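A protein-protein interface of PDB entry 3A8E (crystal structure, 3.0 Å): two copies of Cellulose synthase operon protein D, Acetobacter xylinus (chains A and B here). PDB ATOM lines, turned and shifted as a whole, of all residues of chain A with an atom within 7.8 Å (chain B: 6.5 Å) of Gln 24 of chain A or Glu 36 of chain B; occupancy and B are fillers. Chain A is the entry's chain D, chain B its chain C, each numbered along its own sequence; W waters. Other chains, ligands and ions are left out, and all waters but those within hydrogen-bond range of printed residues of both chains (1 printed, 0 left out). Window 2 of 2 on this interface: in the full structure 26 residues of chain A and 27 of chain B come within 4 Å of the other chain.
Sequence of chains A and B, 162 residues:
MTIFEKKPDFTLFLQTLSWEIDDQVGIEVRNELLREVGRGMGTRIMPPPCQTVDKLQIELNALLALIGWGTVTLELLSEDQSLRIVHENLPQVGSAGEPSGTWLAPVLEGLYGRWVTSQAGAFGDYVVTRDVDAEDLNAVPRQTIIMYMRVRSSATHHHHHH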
ATOM      1  N   THR A  16     -14.962   5.599  25.037  1.00  0.00           N
ATOM      2  CA  THR A  16     -15.180   4.411  24.211  1.00  0.00           C
ATOM      3  C   THR A  16     -15.793   3.249  24.998  1.00  0.00           C
ATOM      4  O   THR A  16     -16.588   2.489  24.443  1.00  0.00           O
ATOM      5  CB  THR A  16     -13.910   3.962  23.441  1.00  0.00           C
ATOM      6  OG1 THR A  16     -12.782   3.965  24.323  1.00  0.00           O
ATOM      7  CG2 THR A  16     -13.628   4.900  22.278  1.00  0.00           C
ATOM      8  N   LEU A  17     -15.445   3.125  26.279  1.00  0.00           N
ATOM      9  CA  LEU A  17     -16.059   2.111  27.134  1.00  0.00           C
ATOM     10  C   LEU A  17     -17.553   2.362  27.312  1.00  0.00           C
ATOM     11  O   LEU A  17     -18.367   1.488  27.011  1.00  0.00           O
ATOM     12  CB  LEU A  17     -15.365   2.012  28.493  1.00  0.00           C
ATOM     13  CG  LEU A  17     -15.908   0.970  29.479  1.00  0.00           C
ATOM     14  CD1 LEU A  17     -15.680  -0.456  28.991  1.00  0.00           C
ATOM     15  CD2 LEU A  17     -15.272   1.172  30.834  1.00  0.00           C
ATOM     16  N   SER A  18     -17.909   3.553  27.786  1.00  0.00           N
ATOM     17  CA  SER A  18     -19.311   3.931  27.932  1.00  0.00           C
ATOM     18  C   SER A  18     -20.095   3.550  26.682  1.00  0.00           C
ATOM     19  O   SER A  18     -21.104   2.848  26.761  1.00  0.00           O
ATOM     20  CB  SER A  18     -19.451   5.429  28.206  1.00  0.00           C
ATOM     21  OG  SER A  18     -18.961   6.201  27.124  1.00  0.00           O
ATOM     22  N   TRP A  19     -19.596   4.006  25.533  1.00  0.00           N
ATOM     23  CA  TRP A  19     -20.194   3.750  24.227  1.00  0.00           C
ATOM     24  C   TRP A  19     -20.362   2.272  23.933  1.00  0.00           C
ATOM     25  O   TRP A  19     -21.472   1.799  23.670  1.00  0.00           O
ATOM     26  CB  TRP A  19     -19.311   4.353  23.146  1.00  0.00           C
ATOM     27  CG  TRP A  19     -19.862   5.583  22.535  1.00  0.00           C
ATOM     28  CD1 TRP A  19     -19.952   6.825  23.108  1.00  0.00           C
ATOM     29  CD2 TRP A  19     -20.388   5.708  21.214  1.00  0.00           C
ATOM     30  NE1 TRP A  19     -20.511   7.714  22.220  1.00  0.00           N
ATOM     31  CE2 TRP A  19     -20.786   7.057  21.049  1.00  0.00           C
ATOM     32  CE3 TRP A  19     -20.564   4.813  20.152  1.00  0.00           C
ATOM     33  CZ2 TRP A  19     -21.351   7.530  19.869  1.00  0.00           C
ATOM     34  CZ3 TRP A  19     -21.124   5.282  18.978  1.00  0.00           C
ATOM     35  CH2 TRP A  19     -21.512   6.631  18.845  1.00  0.00           C
ATOM     36  N   GLU A  20     -19.241   1.554  23.970  1.00  0.00           N
ATOM     37  CA  GLU A  20     -19.235   0.122  23.747  1.00  0.00           C
ATOM     38  C   GLU A  20     -20.258  -0.546  24.647  1.00  0.00           C
ATOM     39  O   GLU A  20     -21.098  -1.316  24.173  1.00  0.00           O
ATOM     40  CB  GLU A  20     -17.843  -0.452  24.005  1.00  0.00           C
ATOM     41  CG  GLU A  20     -17.602  -1.805  23.356  1.00  0.00           C
ATOM     42  CD  GLU A  20     -17.889  -1.810  21.860  1.00  0.00           C
ATOM     43  OE1 GLU A  20     -17.507  -0.843  21.163  1.00  0.00           O
ATOM     44  OE2 GLU A  20     -18.495  -2.790  21.380  1.00  0.00           O
ATOM     45  N   ILE A  21     -20.200  -0.229  25.940  1.00  0.00           N
ATOM     46  CA  ILE A  21     -21.110  -0.830  26.911  1.00  0.00           C
ATOM     47  C   ILE A  21     -22.562  -0.568  26.515  1.00  0.00           C
ATOM     48  O   ILE A  21     -23.347  -1.509  26.406  1.00  0.00           O
ATOM     49  CB  ILE A  21     -20.822  -0.373  28.367  1.00  0.00           C
ATOM     50  CG1 ILE A  21     -19.530  -1.020  28.888  1.00  0.00           C
ATOM     51  CG2 ILE A  21     -21.988  -0.727  29.290  1.00  0.00           C
ATOM     52  CD1 ILE A  21     -19.132  -0.579  30.296  1.00  0.00           C
ATOM     53  N   ASP A  22     -22.890   0.703  26.264  1.00  0.00           N
ATOM     54  CA  ASP A  22     -24.264   1.136  25.959  1.00  0.00           C
ATOM     55  C   ASP A  22     -24.836   0.504  24.703  1.00  0.00           C
ATOM     56  O   ASP A  22     -26.036   0.235  24.609  1.00  0.00           O
ATOM     57  CB  ASP A  22     -24.320   2.654  25.805  1.00  0.00           C
ATOM     58  CG  ASP A  22     -24.245   3.368  27.124  1.00  0.00           C
ATOM     59  OD1 ASP A  22     -23.750   2.763  28.093  1.00  0.00           O
ATOM     60  OD2 ASP A  22     -24.677   4.533  27.197  1.00  0.00           O
ATOM     61  N   ASP A  23     -23.950   0.291  23.741  1.00  0.00           N
ATOM     62  CA  ASP A  23     -24.280  -0.312  22.470  1.00  0.00           C
ATOM     63  C   ASP A  23     -24.629  -1.788  22.666  1.00  0.00           C
ATOM     64  O   ASP A  23     -25.458  -2.340  21.946  1.00  0.00           O
ATOM     65  CB  ASP A  23     -23.069  -0.161  21.546  1.00  0.00           C
ATOM     66  CG  ASP A  23     -23.415  -0.300  20.079  1.00  0.00           C
ATOM     67  OD1 ASP A  23     -22.494  -0.633  19.305  1.00  0.00           O
ATOM     68  OD2 ASP A  23     -24.582  -0.069  19.688  1.00  0.00           O
ATOM     69  N   GLN A  24     -24.001  -2.413  23.659  1.00  0.00           N
ATOM     70  CA  GLN A  24     -24.119  -3.854  23.849  1.00  0.00           C
ATOM     71  C   GLN A  24     -25.107  -4.285  24.926  1.00  0.00           C
ATOM     72  O   GLN A  24     -25.742  -5.326  24.779  1.00  0.00           O
ATOM     73  CB  GLN A  24     -22.750  -4.479  24.123  1.00  0.00           C
ATOM     74  CG  GLN A  24     -21.780  -4.387  22.955  1.00  0.00           C
ATOM     75  CD  GLN A  24     -20.653  -5.393  23.057  1.00  0.00           C
ATOM     76  OE1 GLN A  24     -20.873  -6.602  22.972  1.00  0.00           O
ATOM     77  NE2 GLN A  24     -19.432  -4.898  23.236  1.00  0.00           N
ATOM     78  N   VAL A  25     -25.241  -3.506  25.999  1.00  0.00           N
ATOM     79  CA  VAL A  25     -26.093  -3.921  27.131  1.00  0.00           C
ATOM     80  C   VAL A  25     -27.448  -3.222  27.248  1.00  0.00           C
ATOM     81  O   VAL A  25     -28.433  -3.852  27.630  1.00  0.00           O
ATOM     82  CB  VAL A  25     -25.361  -3.865  28.504  1.00  0.00           C
ATOM     83  CG1 VAL A  25     -24.186  -4.842  28.533  1.00  0.00           C
ATOM     84  CG2 VAL A  25     -24.925  -2.445  28.845  1.00  0.00           C
ATOM     85  N   GLY A  26     -27.496  -1.926  26.944  1.00  0.00           N
ATOM     86  CA  GLY A  26     -28.720  -1.134  27.114  1.00  0.00           C
ATOM     87  C   GLY A  26     -28.623  -0.218  28.322  1.00  0.00           C
ATOM     88  O   GLY A  26     -27.648  -0.290  29.074  1.00  0.00           O
ATOM     89  N   ILE A  27     -29.628   0.635  28.518  1.00  0.00           N
ATOM     90  CA  ILE A  27     -29.594   1.627  29.600  1.00  0.00           C
ATOM     91  C   ILE A  27     -29.755   0.986  30.982  1.00  0.00           C
ATOM     92  O   ILE A  27     -29.038   1.343  31.910  1.00  0.00           O
ATOM     93  CB  ILE A  27     -30.641   2.777  29.411  1.00  0.00           C
ATOM     94  CG1 ILE A  27     -30.684   3.299  27.963  1.00  0.00           C
ATOM     95  CG2 ILE A  27     -30.395   3.922  30.399  1.00  0.00           C
ATOM     96  CD1 ILE A  27     -29.329   3.662  27.351  1.00  0.00           C
ATOM     97  N   VAL A  29     -29.313  -2.254  32.257  1.00  0.00           N
ATOM     98  CA  VAL A  29     -28.266  -3.166  32.716  1.00  0.00           C
ATOM     99  C   VAL A  29     -26.977  -2.401  33.012  1.00  0.00           C
ATOM    100  O   VAL A  29     -26.274  -2.695  33.983  1.00  0.00           O
ATOM    101  CB  VAL A  29     -28.032  -4.310  31.683  1.00  0.00           C
ATOM    102  CG1 VAL A  29     -26.685  -4.991  31.883  1.00  0.00           C
ATOM    103  CG2 VAL A  29     -29.154  -5.331  31.764  1.00  0.00           C
ATOM    104  N   VAL B  29     -15.051 -13.314  27.903  1.00  0.00           N
ATOM    105  CA  VAL B  29     -16.031 -12.284  27.545  1.00  0.00           C
ATOM    106  C   VAL B  29     -15.433 -10.883  27.757  1.00  0.00           C
ATOM    107  O   VAL B  29     -15.440 -10.055  26.842  1.00  0.00           O
ATOM    108  CB  VAL B  29     -17.375 -12.454  28.314  1.00  0.00           C
ATOM    109  CG1 VAL B  29     -18.299 -11.255  28.089  1.00  0.00           C
ATOM    110  CG2 VAL B  29     -18.076 -13.747  27.905  1.00  0.00           C
ATOM    111  N   ASN B  31     -12.306  -9.832  27.919  1.00  0.00           N
ATOM    112  CA  ASN B  31     -11.230  -9.502  26.986  1.00  0.00           C
ATOM    113  C   ASN B  31     -11.769  -9.019  25.649  1.00  0.00           C
ATOM    114  O   ASN B  31     -11.257  -8.046  25.085  1.00  0.00           O
ATOM    115  CB  ASN B  31     -10.291 -10.692  26.777  1.00  0.00           C
ATOM    116  CG  ASN B  31      -9.334 -10.901  27.936  1.00  0.00           C
ATOM    117  OD1 ASN B  31      -9.184 -10.041  28.805  1.00  0.00           O
ATOM    118  ND2 ASN B  31      -8.679 -12.052  27.949  1.00  0.00           N
ATOM    119  N   GLU B  32     -12.810  -9.695  25.158  1.00  0.00           N
ATOM    120  CA  GLU B  32     -13.433  -9.337  23.889  1.00  0.00           C
ATOM    121  C   GLU B  32     -14.083  -7.956  23.948  1.00  0.00           C
ATOM    122  O   GLU B  32     -13.926  -7.153  23.021  1.00  0.00           O
ATOM    123  CB  GLU B  32     -14.428 -10.412  23.432  1.00  0.00           C
ATOM    124  CG  GLU B  32     -14.832 -10.302  21.951  1.00  0.00           C
ATOM    125  CD  GLU B  32     -13.674  -9.875  21.035  1.00  0.00           C
ATOM    126  OE1 GLU B  32     -12.666 -10.612  20.930  1.00  0.00           O
ATOM    127  OE2 GLU B  32     -13.777  -8.795  20.411  1.00  0.00           O
ATOM    128  N   LEU B  33     -14.792  -7.683  25.044  1.00  0.00           N
ATOM    129  CA  LEU B  33     -15.307  -6.346  25.312  1.00  0.00           C
ATOM    130  C   LEU B  33     -14.165  -5.342  25.312  1.00  0.00           C
ATOM    131  O   LEU B  33     -14.288  -4.259  24.743  1.00  0.00           O
ATOM    132  CB  LEU B  33     -16.042  -6.295  26.654  1.00  0.00           C
ATOM    133  CG  LEU B  33     -16.489  -4.923  27.176  1.00  0.00           C
ATOM    134  CD1 LEU B  33     -17.524  -4.264  26.255  1.00  0.00           C
ATOM    135  CD2 LEU B  33     -17.023  -5.050  28.597  1.00  0.00           C
ATOM    136  N   LEU B  34     -13.053  -5.715  25.939  1.00  0.00           N
ATOM    137  CA  LEU B  34     -11.903  -4.822  26.051  1.00  0.00           C
ATOM    138  C   LEU B  34     -11.131  -4.563  24.754  1.00  0.00           C
ATOM    139  O   LEU B  34     -10.598  -3.467  24.576  1.00  0.00           O
ATOM    140  CB  LEU B  34     -10.966  -5.252  27.186  1.00  0.00           C
ATOM    141  CG  LEU B  34     -10.886  -4.344  28.426  1.00  0.00           C
ATOM    142  CD1 LEU B  34     -12.226  -3.727  28.825  1.00  0.00           C
ATOM    143  CD2 LEU B  34     -10.274  -5.097  29.599  1.00  0.00           C
ATOM    144  N   ARG B  35     -11.068  -5.555  23.861  1.00  0.00           N
ATOM    145  CA  ARG B  35     -10.481  -5.353  22.527  1.00  0.00           C
ATOM    146  C   ARG B  35     -11.324  -4.395  21.713  1.00  0.00           C
ATOM    147  O   ARG B  35     -10.799  -3.509  21.039  1.00  0.00           O
ATOM    148  CB  ARG B  35     -10.399  -6.657  21.749  1.00  0.00           C
ATOM    149  CG  ARG B  35      -9.487  -7.673  22.356  1.00  0.00           C
ATOM    150  CD  ARG B  35      -9.248  -8.809  21.390  1.00  0.00           C
ATOM    151  NE  ARG B  35      -8.701  -9.943  22.115  1.00  0.00           N
ATOM    152  CZ  ARG B  35      -9.441 -10.900  22.664  1.00  0.00           C
ATOM    153  NH1 ARG B  35     -10.763 -10.876  22.552  1.00  0.00           N
ATOM    154  NH2 ARG B  35      -8.856 -11.892  23.322  1.00  0.00           N
ATOM    155  N   GLU B  36     -12.638  -4.614  21.757  1.00  0.00           N
ATOM    156  CA  GLU B  36     -13.602  -3.758  21.079  1.00  0.00           C
ATOM    157  C   GLU B  36     -13.367  -2.309  21.476  1.00  0.00           C
ATOM    158  O   GLU B  36     -13.307  -1.420  20.622  1.00  0.00           O
ATOM    159  CB  GLU B  36     -15.032  -4.176  21.426  1.00  0.00           C
ATOM    160  CG  GLU B  36     -15.562  -5.336  20.598  1.00  0.00           C
ATOM    161  CD  GLU B  36     -16.683  -6.105  21.296  1.00  0.00           C
ATOM    162  OE1 GLU B  36     -17.063  -5.733  22.429  1.00  0.00           O
ATOM    163  OE2 GLU B  36     -17.181  -7.093  20.708  1.00  0.00           O
ATOM    164  N   VAL B  37     -13.219  -2.081  22.775  1.00  0.00           N
ATOM    165  CA  VAL B  37     -12.956  -0.746  23.275  1.00  0.00           C
ATOM    166  C   VAL B  37     -11.635  -0.222  22.695  1.00  0.00           C
ATOM    167  O   VAL B  37     -11.525   0.964  22.374  1.00  0.00           O
ATOM    168  CB  VAL B  37     -13.011  -0.697  24.822  1.00  0.00           C
ATOM    169  CG1 VAL B  37     -12.370   0.565  25.363  1.00  0.00           C
ATOM    170  CG2 VAL B  37     -14.450  -0.785  25.290  1.00  0.00           C
ATOM    171  N   GLY B  38     -10.660  -1.118  22.528  1.00  0.00           N
ATOM    172  CA  GLY B  38      -9.392  -0.787  21.873  1.00  0.00           C
ATOM    173  C   GLY B  38      -9.587  -0.310  20.442  1.00  0.00           C
ATOM    174  O   GLY B  38      -9.146   0.787  20.087  1.00  0.00           O
ATOM    175  N   ARG B  39     -10.246  -1.135  19.624  1.00  0.00           N
ATOM    176  CA  ARG B  39     -10.652  -0.737  18.273  1.00  0.00           C
ATOM    177  C   ARG B  39     -11.260   0.662  18.278  1.00  0.00           C
ATOM    178  O   ARG B  39     -10.899   1.503  17.455  1.00  0.00           O
ATOM    179  CB  ARG B  39     -11.678  -1.714  17.688  1.00  0.00           C
ATOM    180  CG  ARG B  39     -11.104  -2.847  16.858  1.00  0.00           C
ATOM    181  CD  ARG B  39     -11.724  -2.902  15.448  1.00  0.00           C
ATOM    182  NE  ARG B  39     -13.127  -2.468  15.382  1.00  0.00           N
ATOM    183  CZ  ARG B  39     -13.546  -1.330  14.826  1.00  0.00           C
ATOM    184  NH1 ARG B  39     -12.679  -0.485  14.274  1.00  0.00           N
ATOM    185  NH2 ARG B  39     -14.841  -1.032  14.820  1.00  0.00           N
ATOM    186  N   GLY B  40     -12.181   0.895  19.214  1.00  0.00           N
ATOM    187  CA  GLY B  40     -12.872   2.173  19.340  1.00  0.00           C
ATOM    188  C   GLY B  40     -11.909   3.312  19.588  1.00  0.00           C
ATOM    189  O   GLY B  40     -11.957   4.334  18.900  1.00  0.00           O
ATOM    190  N   MET B  41     -11.027   3.123  20.568  1.00  0.00           N
ATOM    191  CA  MET B  41     -10.009   4.113  20.895  1.00  0.00           C
ATOM    192  C   MET B  41      -9.152   4.456  19.686  1.00  0.00           C
ATOM    193  O   MET B  41      -8.821   5.620  19.455  1.00  0.00           O
ATOM    194  CB  MET B  41      -9.140   3.632  22.055  1.00  0.00           C
ATOM    195  CG  MET B  41      -9.668   4.082  23.399  1.00  0.00           C
ATOM    196  SD  MET B  41      -8.884   3.265  24.785  1.00  0.00           S
ATOM    197  CE  MET B  41      -7.379   4.226  24.933  1.00  0.00           C
ATOM    198  N   PRO B 106      -5.840  -6.185  27.043  1.00  0.00           N
ATOM    199  CA  PRO B 106      -6.477  -6.442  25.754  1.00  0.00           C
ATOM    200  C   PRO B 106      -6.933  -5.178  25.025  1.00  0.00           C
ATOM    201  O   PRO B 106      -7.270  -5.254  23.842  1.00  0.00           O
ATOM    202  CB  PRO B 106      -7.689  -7.312  26.121  1.00  0.00           C
ATOM    203  CG  PRO B 106      -7.396  -7.835  27.479  1.00  0.00           C
ATOM    204  CD  PRO B 106      -6.636  -6.743  28.147  1.00  0.00           C
ATOM    205  N   GLY B 110      -6.753  -4.352  20.909  1.00  0.00           N
ATOM    206  CA  GLY B 110      -7.694  -3.627  20.078  1.00  0.00           C
ATOM    207  C   GLY B 110      -7.007  -2.420  19.481  1.00  0.00           C
ATOM    208  O   GLY B 110      -6.996  -2.245  18.264  1.00  0.00           O
HETATM  209  O   HOH W   1     -18.320  -7.895  23.400  1.00  0.00           O
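The side-chain carboxylate (OE1) of Glu 36 of chain B is in hydrogen-bond range of the side-chain amide nitrogen (NE2) of Gln 24 of chain A, at 2.6 Å.
The side-chain carboxylate (OE2) of Glu 20 of chain A sits close to the side-chain carboxylate (OE1) of Glu 36 of chain B (3.4 Å).
The side-chain carboxylate of Glu 20 of chain A sits at hydrogen-bond distance from the side-chain amide nitrogen of Gln 24 of chain A (3.0 Å).
OG1 of Thr 16 of chain A touches CG1 of Val 37 of chain B, 3.6 Å away.
C of Gly 40 of chain B touches CG2 of Thr 16 of chain A, 3.6 Å away.
Thr 16 of chain A touches Met 41 of chain B.
Val 37 of chain B touches Leu 17 of chain A.
Glu 20 of chain A touches Leu 33 of chain B.
Val 37 of chain B touches Glu 20 of chain A.
Gln 24 of chain A touches Leu 33 of chain B.
Of the printed residues of chain B, Leu 17 of chain A touches Val 37.
Printed residues of chain B within 4 Å of Glu 20 of chain A: Leu 33 (3.8 Å), Glu 36 (3.4 Å) and Val 37 (3.6 Å).
Of chain B, only Leu 33 (3.6 Å) and Glu 36 (2.6 Å) come within 4 Å of Gln 24 of chain A.
Glu 36 of chain B touches just these residues of chain A: Glu 20 and Gln 24.
Of the printed residues of chain A, Gly 40 of chain B touches Thr 16 (3.6 Å).
Of the printed residues of chain A, Met 41 of chain B touches Thr 16 (3.3 Å).
Hydrophobic or aromatic side chains of chain B within 4 Å of the printed part of chain A: Leu 33, Val 37 and Met 41.
Hydrophobic or aromatic side chains of chain A that line the printed part of chain B: Leu 17.
Among the printed residues, 9 pairs touch across the chains.
1 position is printed for both chains.
Of the 9 pairs that touch across the chains among the printed residues, none has its exchanged pair printed and touching as well.
Water W1 lies within hydrogen-bond range of OE1 of Glu 36 of chain B (2.7 Å) and OE1 of Gln 24 of chain A (2.9 Å).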
